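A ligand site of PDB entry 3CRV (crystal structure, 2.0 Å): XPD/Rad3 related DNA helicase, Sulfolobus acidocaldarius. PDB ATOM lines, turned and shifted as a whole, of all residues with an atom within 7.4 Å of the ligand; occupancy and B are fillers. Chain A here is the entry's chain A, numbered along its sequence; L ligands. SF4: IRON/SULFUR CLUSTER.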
ATOM      1  N   LYS A  84     -25.851  25.747  -1.318  1.00  0.00           N
ATOM      2  CA  LYS A  84     -25.675  25.880   0.091  1.00  0.00           C
ATOM      3  C   LYS A  84     -24.340  25.360   0.581  1.00  0.00           C
ATOM      4  O   LYS A  84     -23.752  25.946   1.393  1.00  0.00           O
ATOM      5  CB  LYS A  84     -26.803  25.158   0.818  1.00  0.00           C
ATOM      6  CG  LYS A  84     -26.836  25.324   2.323  1.00  0.00           C
ATOM      7  CD  LYS A  84     -27.703  24.289   2.982  1.00  0.00           C
ATOM      8  CE  LYS A  84     -29.043  24.283   2.395  1.00  0.00           C
ATOM      9  NZ  LYS A  84     -30.066  23.746   3.200  1.00  0.00           N
ATOM     10  N   PRO A  85     -23.756  24.380  -0.097  1.00  0.00           N
ATOM     11  CA  PRO A  85     -22.466  24.138   0.551  1.00  0.00           C
ATOM     12  C   PRO A  85     -21.593  25.395   0.182  1.00  0.00           C
ATOM     13  O   PRO A  85     -20.526  25.628   0.767  1.00  0.00           O
ATOM     14  CB  PRO A  85     -21.970  22.857  -0.135  1.00  0.00           C
ATOM     15  CG  PRO A  85     -22.708  22.840  -1.449  1.00  0.00           C
ATOM     16  CD  PRO A  85     -24.080  23.323  -1.074  1.00  0.00           C
ATOM     17  N   SER A  87     -22.875  28.838   0.117  1.00  0.00           N
ATOM     18  CA  SER A  87     -23.305  30.059   0.777  1.00  0.00           C
ATOM     19  C   SER A  87     -23.400  29.962   2.302  1.00  0.00           C
ATOM     20  O   SER A  87     -23.498  30.979   2.988  1.00  0.00           O
ATOM     21  CB  SER A  87     -24.648  30.518   0.208  1.00  0.00           C
ATOM     22  OG  SER A  87     -25.515  29.400   0.019  1.00  0.00           O
ATOM     23  N   CYS A  88     -23.361  28.735   2.817  1.00  0.00           N
ATOM     24  CA  CYS A  88     -23.427  28.505   4.241  1.00  0.00           C
ATOM     25  C   CYS A  88     -22.216  29.116   4.932  1.00  0.00           C
ATOM     26  O   CYS A  88     -21.083  28.978   4.471  1.00  0.00           O
ATOM     27  CB  CYS A  88     -23.472  27.002   4.548  1.00  0.00           C
ATOM     28  SG  CYS A  88     -23.448  26.647   6.311  1.00  0.00           S
ATOM     29  N   LEU A  89     -22.456  29.799   6.041  1.00  0.00           N
ATOM     30  CA  LEU A  89     -21.386  30.440   6.802  1.00  0.00           C
ATOM     31  C   LEU A  89     -20.410  29.442   7.428  1.00  0.00           C
ATOM     32  O   LEU A  89     -19.238  29.757   7.622  1.00  0.00           O
ATOM     33  CB  LEU A  89     -22.001  31.312   7.910  1.00  0.00           C
ATOM     34  CG  LEU A  89     -22.069  32.830   7.767  1.00  0.00           C
ATOM     35  CD1 LEU A  89     -22.474  33.232   6.364  1.00  0.00           C
ATOM     36  CD2 LEU A  89     -23.045  33.380   8.799  1.00  0.00           C
ATOM     37  N   TYR A  90     -20.897  28.240   7.722  1.00  0.00           N
ATOM     38  CA  TYR A  90     -20.072  27.223   8.370  1.00  0.00           C
ATOM     39  C   TYR A  90     -19.717  26.014   7.525  1.00  0.00           C
ATOM     40  O   TYR A  90     -19.294  24.979   8.056  1.00  0.00           O
ATOM     41  CB  TYR A  90     -20.773  26.744   9.641  1.00  0.00           C
ATOM     42  CG  TYR A  90     -21.407  27.867  10.427  1.00  0.00           C
ATOM     43  CD1 TYR A  90     -22.785  27.929  10.612  1.00  0.00           C
ATOM     44  CD2 TYR A  90     -20.614  28.874  10.988  1.00  0.00           C
ATOM     45  CE1 TYR A  90     -23.372  28.962  11.336  1.00  0.00           C
ATOM     46  CE2 TYR A  90     -21.191  29.916  11.715  1.00  0.00           C
ATOM     47  CZ  TYR A  90     -22.570  29.950  11.886  1.00  0.00           C
ATOM     48  OH  TYR A  90     -23.136  30.973  12.602  1.00  0.00           O
ATOM     49  N   ALA A  91     -19.878  26.121   6.214  1.00  0.00           N
ATOM     50  CA  ALA A  91     -19.578  25.005   5.329  1.00  0.00           C
ATOM     51  C   ALA A  91     -18.155  25.034   4.800  1.00  0.00           C
ATOM     52  O   ALA A  91     -17.658  26.074   4.367  1.00  0.00           O
ATOM     53  CB  ALA A  91     -20.556  25.004   4.161  1.00  0.00           C
ATOM     54  N   ILE A 100     -25.498  19.961   5.712  1.00  0.00           N
ATOM     55  CA  ILE A 100     -25.635  21.213   6.440  1.00  0.00           C
ATOM     56  C   ILE A 100     -26.826  21.128   7.396  1.00  0.00           C
ATOM     57  O   ILE A 100     -27.980  21.166   6.971  1.00  0.00           O
ATOM     58  CB  ILE A 100     -25.868  22.396   5.463  1.00  0.00           C
ATOM     59  CG1 ILE A 100     -24.909  22.304   4.273  1.00  0.00           C
ATOM     60  CG2 ILE A 100     -25.692  23.729   6.191  1.00  0.00           C
ATOM     61  CD1 ILE A 100     -23.447  22.371   4.645  1.00  0.00           C
ATOM     62  N   PRO A 101     -26.561  20.988   8.706  1.00  0.00           N
ATOM     63  CA  PRO A 101     -27.597  20.889   9.746  1.00  0.00           C
ATOM     64  C   PRO A 101     -28.301  22.210  10.087  1.00  0.00           C
ATOM     65  O   PRO A 101     -28.302  22.644  11.243  1.00  0.00           O
ATOM     66  CB  PRO A 101     -26.823  20.331  10.931  1.00  0.00           C
ATOM     67  CG  PRO A 101     -25.515  21.030  10.795  1.00  0.00           C
ATOM     68  CD  PRO A 101     -25.218  20.893   9.309  1.00  0.00           C
ATOM     69  N   CYS A 102     -28.899  22.832   9.076  1.00  0.00           N
ATOM     70  CA  CYS A 102     -29.600  24.098   9.257  1.00  0.00           C
ATOM     71  C   CYS A 102     -30.568  24.074  10.452  1.00  0.00           C
ATOM     72  O   CYS A 102     -30.775  25.095  11.112  1.00  0.00           O
ATOM     73  CB  CYS A 102     -30.338  24.481   7.969  1.00  0.00           C
ATOM     74  SG  CYS A 102     -29.254  24.740   6.514  1.00  0.00           S
ATOM     75  N   LYS A 103     -31.146  22.907  10.727  1.00  0.00           N
ATOM     76  CA  LYS A 103     -32.082  22.785  11.843  1.00  0.00           C
ATOM     77  C   LYS A 103     -31.497  23.308  13.150  1.00  0.00           C
ATOM     78  O   LYS A 103     -32.151  24.028  13.888  1.00  0.00           O
ATOM     79  CB  LYS A 103     -32.487  21.320  12.055  1.00  0.00           C
ATOM     80  CG  LYS A 103     -33.358  20.737  10.966  1.00  0.00           C
ATOM     81  CD  LYS A 103     -34.011  19.447  11.439  1.00  0.00           C
ATOM     82  CE  LYS A 103     -34.987  19.704  12.580  1.00  0.00           C
ATOM     83  NZ  LYS A 103     -35.621  18.458  13.091  1.00  0.00           N
ATOM     84  N   TYR A 104     -30.249  22.928  13.428  1.00  0.00           N
ATOM     85  CA  TYR A 104     -29.590  23.331  14.670  1.00  0.00           C
ATOM     86  C   TYR A 104     -28.890  24.672  14.595  1.00  0.00           C
ATOM     87  O   TYR A 104     -28.146  25.042  15.508  1.00  0.00           O
ATOM     88  CB  TYR A 104     -28.590  22.248  15.091  1.00  0.00           C
ATOM     89  CG  TYR A 104     -29.172  20.855  15.022  1.00  0.00           C
ATOM     90  CD1 TYR A 104     -29.215  20.151  13.818  1.00  0.00           C
ATOM     91  CD2 TYR A 104     -29.720  20.258  16.152  1.00  0.00           C
ATOM     92  CE1 TYR A 104     -29.791  18.888  13.745  1.00  0.00           C
ATOM     93  CE2 TYR A 104     -30.313  18.999  16.093  1.00  0.00           C
ATOM     94  CZ  TYR A 104     -30.342  18.326  14.883  1.00  0.00           C
ATOM     95  OH  TYR A 104     -30.927  17.090  14.829  1.00  0.00           O
ATOM     96  N   CYS A 105     -29.121  25.401  13.516  1.00  0.00           N
ATOM     97  CA  CYS A 105     -28.490  26.708  13.332  1.00  0.00           C
ATOM     98  C   CYS A 105     -29.436  27.820  13.762  1.00  0.00           C
ATOM     99  O   CYS A 105     -30.618  27.798  13.432  1.00  0.00           O
ATOM    100  CB  CYS A 105     -28.084  26.897  11.868  1.00  0.00           C
ATOM    101  SG  CYS A 105     -27.131  28.386  11.564  1.00  0.00           S
ATOM    102  N   GLU A 106     -28.912  28.802  14.488  1.00  0.00           N
ATOM    103  CA  GLU A 106     -29.724  29.919  14.956  1.00  0.00           C
ATOM    104  C   GLU A 106     -29.896  30.995  13.888  1.00  0.00           C
ATOM    105  O   GLU A 106     -30.363  32.108  14.178  1.00  0.00           O
ATOM    106  CB  GLU A 106     -29.109  30.529  16.213  1.00  0.00           C
ATOM    107  CG  GLU A 106     -27.604  30.727  16.143  1.00  0.00           C
ATOM    108  CD  GLU A 106     -27.033  31.249  17.439  1.00  0.00           C
ATOM    109  OE1 GLU A 106     -27.322  32.410  17.788  1.00  0.00           O
ATOM    110  OE2 GLU A 106     -26.288  30.497  18.122  1.00  0.00           O
ATOM    111  N   LEU A 107     -29.533  30.670  12.651  1.00  0.00           N
ATOM    112  CA  LEU A 107     -29.660  31.605  11.545  1.00  0.00           C
ATOM    113  C   LEU A 107     -30.669  31.081  10.523  1.00  0.00           C
ATOM    114  O   LEU A 107     -30.975  31.744   9.527  1.00  0.00           O
ATOM    115  CB  LEU A 107     -28.300  31.825  10.863  1.00  0.00           C
ATOM    116  CG  LEU A 107     -27.326  32.814  11.520  1.00  0.00           C
ATOM    117  CD1 LEU A 107     -27.266  32.587  13.017  1.00  0.00           C
ATOM    118  CD2 LEU A 107     -25.958  32.659  10.901  1.00  0.00           C
ATOM    119  N   LYS A 108     -31.179  29.883  10.789  1.00  0.00           N
ATOM    120  CA  LYS A 108     -32.154  29.214   9.923  1.00  0.00           C
ATOM    121  C   LYS A 108     -33.295  30.132   9.452  1.00  0.00           C
ATOM    122  O   LYS A 108     -33.821  29.959   8.354  1.00  0.00           O
ATOM    123  CB  LYS A 108     -32.728  28.002  10.660  1.00  0.00           C
ATOM    124  CG  LYS A 108     -33.215  28.305  12.074  1.00  0.00           C
ATOM    125  CD  LYS A 108     -33.412  27.042  12.916  1.00  0.00           C
ATOM    126  CE  LYS A 108     -34.540  26.164  12.393  1.00  0.00           C
ATOM    127  NZ  LYS A 108     -34.772  24.966  13.263  1.00  0.00           N
ATOM    128  N   GLY A 109     -33.656  31.105  10.279  1.00  0.00           N
ATOM    129  CA  GLY A 109     -34.726  32.016   9.902  1.00  0.00           C
ATOM    130  C   GLY A 109     -34.296  33.450   9.658  1.00  0.00           C
ATOM    131  O   GLY A 109     -35.082  34.263   9.179  1.00  0.00           O
ATOM    132  N   SER A 110     -33.046  33.763   9.996  1.00  0.00           N
ATOM    133  CA  SER A 110     -32.525  35.115   9.831  1.00  0.00           C
ATOM    134  C   SER A 110     -32.046  35.408   8.406  1.00  0.00           C
ATOM    135  O   SER A 110     -31.044  34.867   7.948  1.00  0.00           O
ATOM    136  CB  SER A 110     -31.374  35.370  10.808  1.00  0.00           C
ATOM    137  OG  SER A 110     -31.805  35.177  12.153  1.00  0.00           O
ATOM    138  N   PHE A 136     -26.782  36.535   9.817  1.00  0.00           N
ATOM    139  CA  PHE A 136     -27.846  36.110   8.923  1.00  0.00           C
ATOM    140  C   PHE A 136     -27.333  35.050   7.940  1.00  0.00           C
ATOM    141  O   PHE A 136     -26.133  34.978   7.657  1.00  0.00           O
ATOM    142  CB  PHE A 136     -28.433  37.316   8.166  1.00  0.00           C
ATOM    143  CG  PHE A 136     -27.509  37.920   7.140  1.00  0.00           C
ATOM    144  CD1 PHE A 136     -27.202  37.245   5.952  1.00  0.00           C
ATOM    145  CD2 PHE A 136     -26.960  39.179   7.338  1.00  0.00           C
ATOM    146  CE1 PHE A 136     -26.378  37.821   4.989  1.00  0.00           C
ATOM    147  CE2 PHE A 136     -26.137  39.776   6.382  1.00  0.00           C
ATOM    148  CZ  PHE A 136     -25.845  39.091   5.207  1.00  0.00           C
ATOM    149  N   CYS A 137     -28.243  34.236   7.422  1.00  0.00           N
ATOM    150  CA  CYS A 137     -27.877  33.177   6.481  1.00  0.00           C
ATOM    151  C   CYS A 137     -27.939  33.638   5.036  1.00  0.00           C
ATOM    152  O   CYS A 137     -29.023  33.944   4.527  1.00  0.00           O
ATOM    153  CB  CYS A 137     -28.781  31.955   6.649  1.00  0.00           C
ATOM    154  SG  CYS A 137     -28.418  30.658   5.446  1.00  0.00           S
ATOM    155  N   PRO A 138     -26.786  33.667   4.346  1.00  0.00           N
ATOM    156  CA  PRO A 138     -26.735  34.087   2.948  1.00  0.00           C
ATOM    157  C   PRO A 138     -27.599  33.229   2.050  1.00  0.00           C
ATOM    158  O   PRO A 138     -28.304  33.739   1.187  1.00  0.00           O
ATOM    159  CB  PRO A 138     -25.240  33.946   2.605  1.00  0.00           C
ATOM    160  CG  PRO A 138     -24.569  34.204   3.919  1.00  0.00           C
ATOM    161  CD  PRO A 138     -25.432  33.406   4.870  1.00  0.00           C
ATOM    162  N   TYR A 139     -27.555  31.919   2.260  1.00  0.00           N
ATOM    163  CA  TYR A 139     -28.336  30.991   1.459  1.00  0.00           C
ATOM    164  C   TYR A 139     -29.821  31.309   1.492  1.00  0.00           C
ATOM    165  O   TYR A 139     -30.436  31.541   0.446  1.00  0.00           O
ATOM    166  CB  TYR A 139     -28.139  29.563   1.945  1.00  0.00           C
ATOM    167  CG  TYR A 139     -29.019  28.564   1.221  1.00  0.00           C
ATOM    168  CD1 TYR A 139     -28.775  28.223  -0.106  1.00  0.00           C
ATOM    169  CD2 TYR A 139     -30.103  27.968   1.868  1.00  0.00           C
ATOM    170  CE1 TYR A 139     -29.588  27.319  -0.782  1.00  0.00           C
ATOM    171  CE2 TYR A 139     -30.922  27.055   1.203  1.00  0.00           C
ATOM    172  CZ  TYR A 139     -30.657  26.732  -0.118  1.00  0.00           C
ATOM    173  OH  TYR A 139     -31.451  25.823  -0.777  1.00  0.00           O
ATOM    174  N   TYR A 140     -30.404  31.313   2.682  1.00  0.00           N
ATOM    175  CA  TYR A 140     -31.821  31.600   2.818  1.00  0.00           C
ATOM    176  C   TYR A 140     -32.170  33.003   2.346  1.00  0.00           C
ATOM    177  O   TYR A 140     -33.275  33.253   1.869  1.00  0.00           O
ATOM    178  CB  TYR A 140     -32.282  31.360   4.259  1.00  0.00           C
ATOM    179  CG  TYR A 140     -32.433  29.876   4.555  1.00  0.00           C
ATOM    180  CD1 TYR A 140     -31.567  29.235   5.432  1.00  0.00           C
ATOM    181  CD2 TYR A 140     -33.382  29.115   3.877  1.00  0.00           C
ATOM    182  CE1 TYR A 140     -31.643  27.848   5.630  1.00  0.00           C
ATOM    183  CE2 TYR A 140     -33.463  27.727   4.062  1.00  0.00           C
ATOM    184  CZ  TYR A 140     -32.581  27.103   4.933  1.00  0.00           C
ATOM    185  OH  TYR A 140     -32.642  25.742   5.101  1.00  0.00           O
ATOM    186  N   LEU A 263     -21.701  21.411  13.324  1.00  0.00           N
ATOM    187  CA  LEU A 263     -22.302  22.741  13.291  1.00  0.00           C
ATOM    188  C   LEU A 263     -21.902  23.480  14.561  1.00  0.00           C
ATOM    189  O   LEU A 263     -21.814  24.707  14.566  1.00  0.00           O
ATOM    190  CB  LEU A 263     -23.832  22.627  13.196  1.00  0.00           C
ATOM    191  CG  LEU A 263     -24.656  23.918  13.046  1.00  0.00           C
ATOM    192  CD1 LEU A 263     -24.782  24.637  14.383  1.00  0.00           C
ATOM    193  CD2 LEU A 263     -24.009  24.807  12.003  1.00  0.00           C
ATOM    194  N   VAL A 268     -18.498  22.527   9.027  1.00  0.00           N
ATOM    195  CA  VAL A 268     -19.225  21.434   8.397  1.00  0.00           C
ATOM    196  C   VAL A 268     -18.433  20.845   7.239  1.00  0.00           C
ATOM    197  O   VAL A 268     -18.331  21.464   6.176  1.00  0.00           O
ATOM    198  CB  VAL A 268     -20.589  21.895   7.859  1.00  0.00           C
ATOM    199  CG1 VAL A 268     -21.390  20.695   7.379  1.00  0.00           C
ATOM    200  CG2 VAL A 268     -21.333  22.676   8.927  1.00  0.00           C
HETATM  201 FE1  SF4 L   1     -27.584  29.074   6.794  1.00  0.00          FE
HETATM  202 FE2  SF4 L   1     -27.003  28.151   9.234  1.00  0.00          FE
HETATM  203 FE3  SF4 L   1     -25.431  27.354   7.155  1.00  0.00          FE
HETATM  204 FE4  SF4 L   1     -27.976  26.542   7.279  1.00  0.00          FE
HETATM  205  S1  SF4 L   1     -26.326  26.065   8.738  1.00  0.00           S
HETATM  206  S2  SF4 L   1     -27.145  27.318   5.423  1.00  0.00           S
HETATM  207  S3  SF4 L   1     -29.101  28.288   8.309  1.00  0.00           S
HETATM  208  S4  SF4 L   1     -25.590  29.521   8.041  1.00  0.00           S
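An iron atom (FE1) of the ligand is bound by the side-chain sulfur (SG) of Cys 137 (2.2 Å).
The side-chain sulfur of Cys 88 is bound to an iron atom (FE3) of the ligand, at 2.3 Å.
An iron atom (FE4) of the ligand is bound by the side-chain sulfur (SG) of Cys 102.
The side-chain sulfur (SG) of Cys 105 binds an iron atom (FE2) of the ligand (2.3 Å).
The backbone NH (N) of Lys 108 sits close to a sulfur (S3) of the ligand (3.6 Å).
A sulfur (S4) of the ligand sits close to the backbone NH (N) of Leu 89.
SG of Cys 137 lies close to N of Tyr 140 (3.5 Å).
The side-chain sulfur (SG) of Cys 137 sits close to the backbone NH (N) of Tyr 139 (3.5 Å).
N of Cys 137 sits at hydrogen-bond distance from O of Ser 110.
The side-chain sulfur (SG) of Cys 88 sits close to the backbone NH (N) of Tyr 90 (3.3 Å).
The side-chain sulfur of Cys 88 sits close to the backbone NH of Ala 91, at 3.6 Å.
The side-chain sulfur (SG) of Cys 102 sits close to the side-chain amino group (NZ) of Lys 84, 3.6 Å away.
The side-chain sulfur of Cys 105 lies close to the backbone NH of Leu 107.
The side-chain amino group (NZ) of Lys 108 sits at hydrogen-bond distance from the backbone carbonyl oxygen (O) of Lys 103, 2.9 Å away.
Merely in contact with the ligand: Ile 100, Lys 84, Tyr 140 and Leu 107.
Hydrophobic or aromatic side chains within 4 Å of the ligand: Ile 100 and Tyr 140.
The nearest printed residue that does not touch the ligand is Tyr 90 (4.01 Å).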
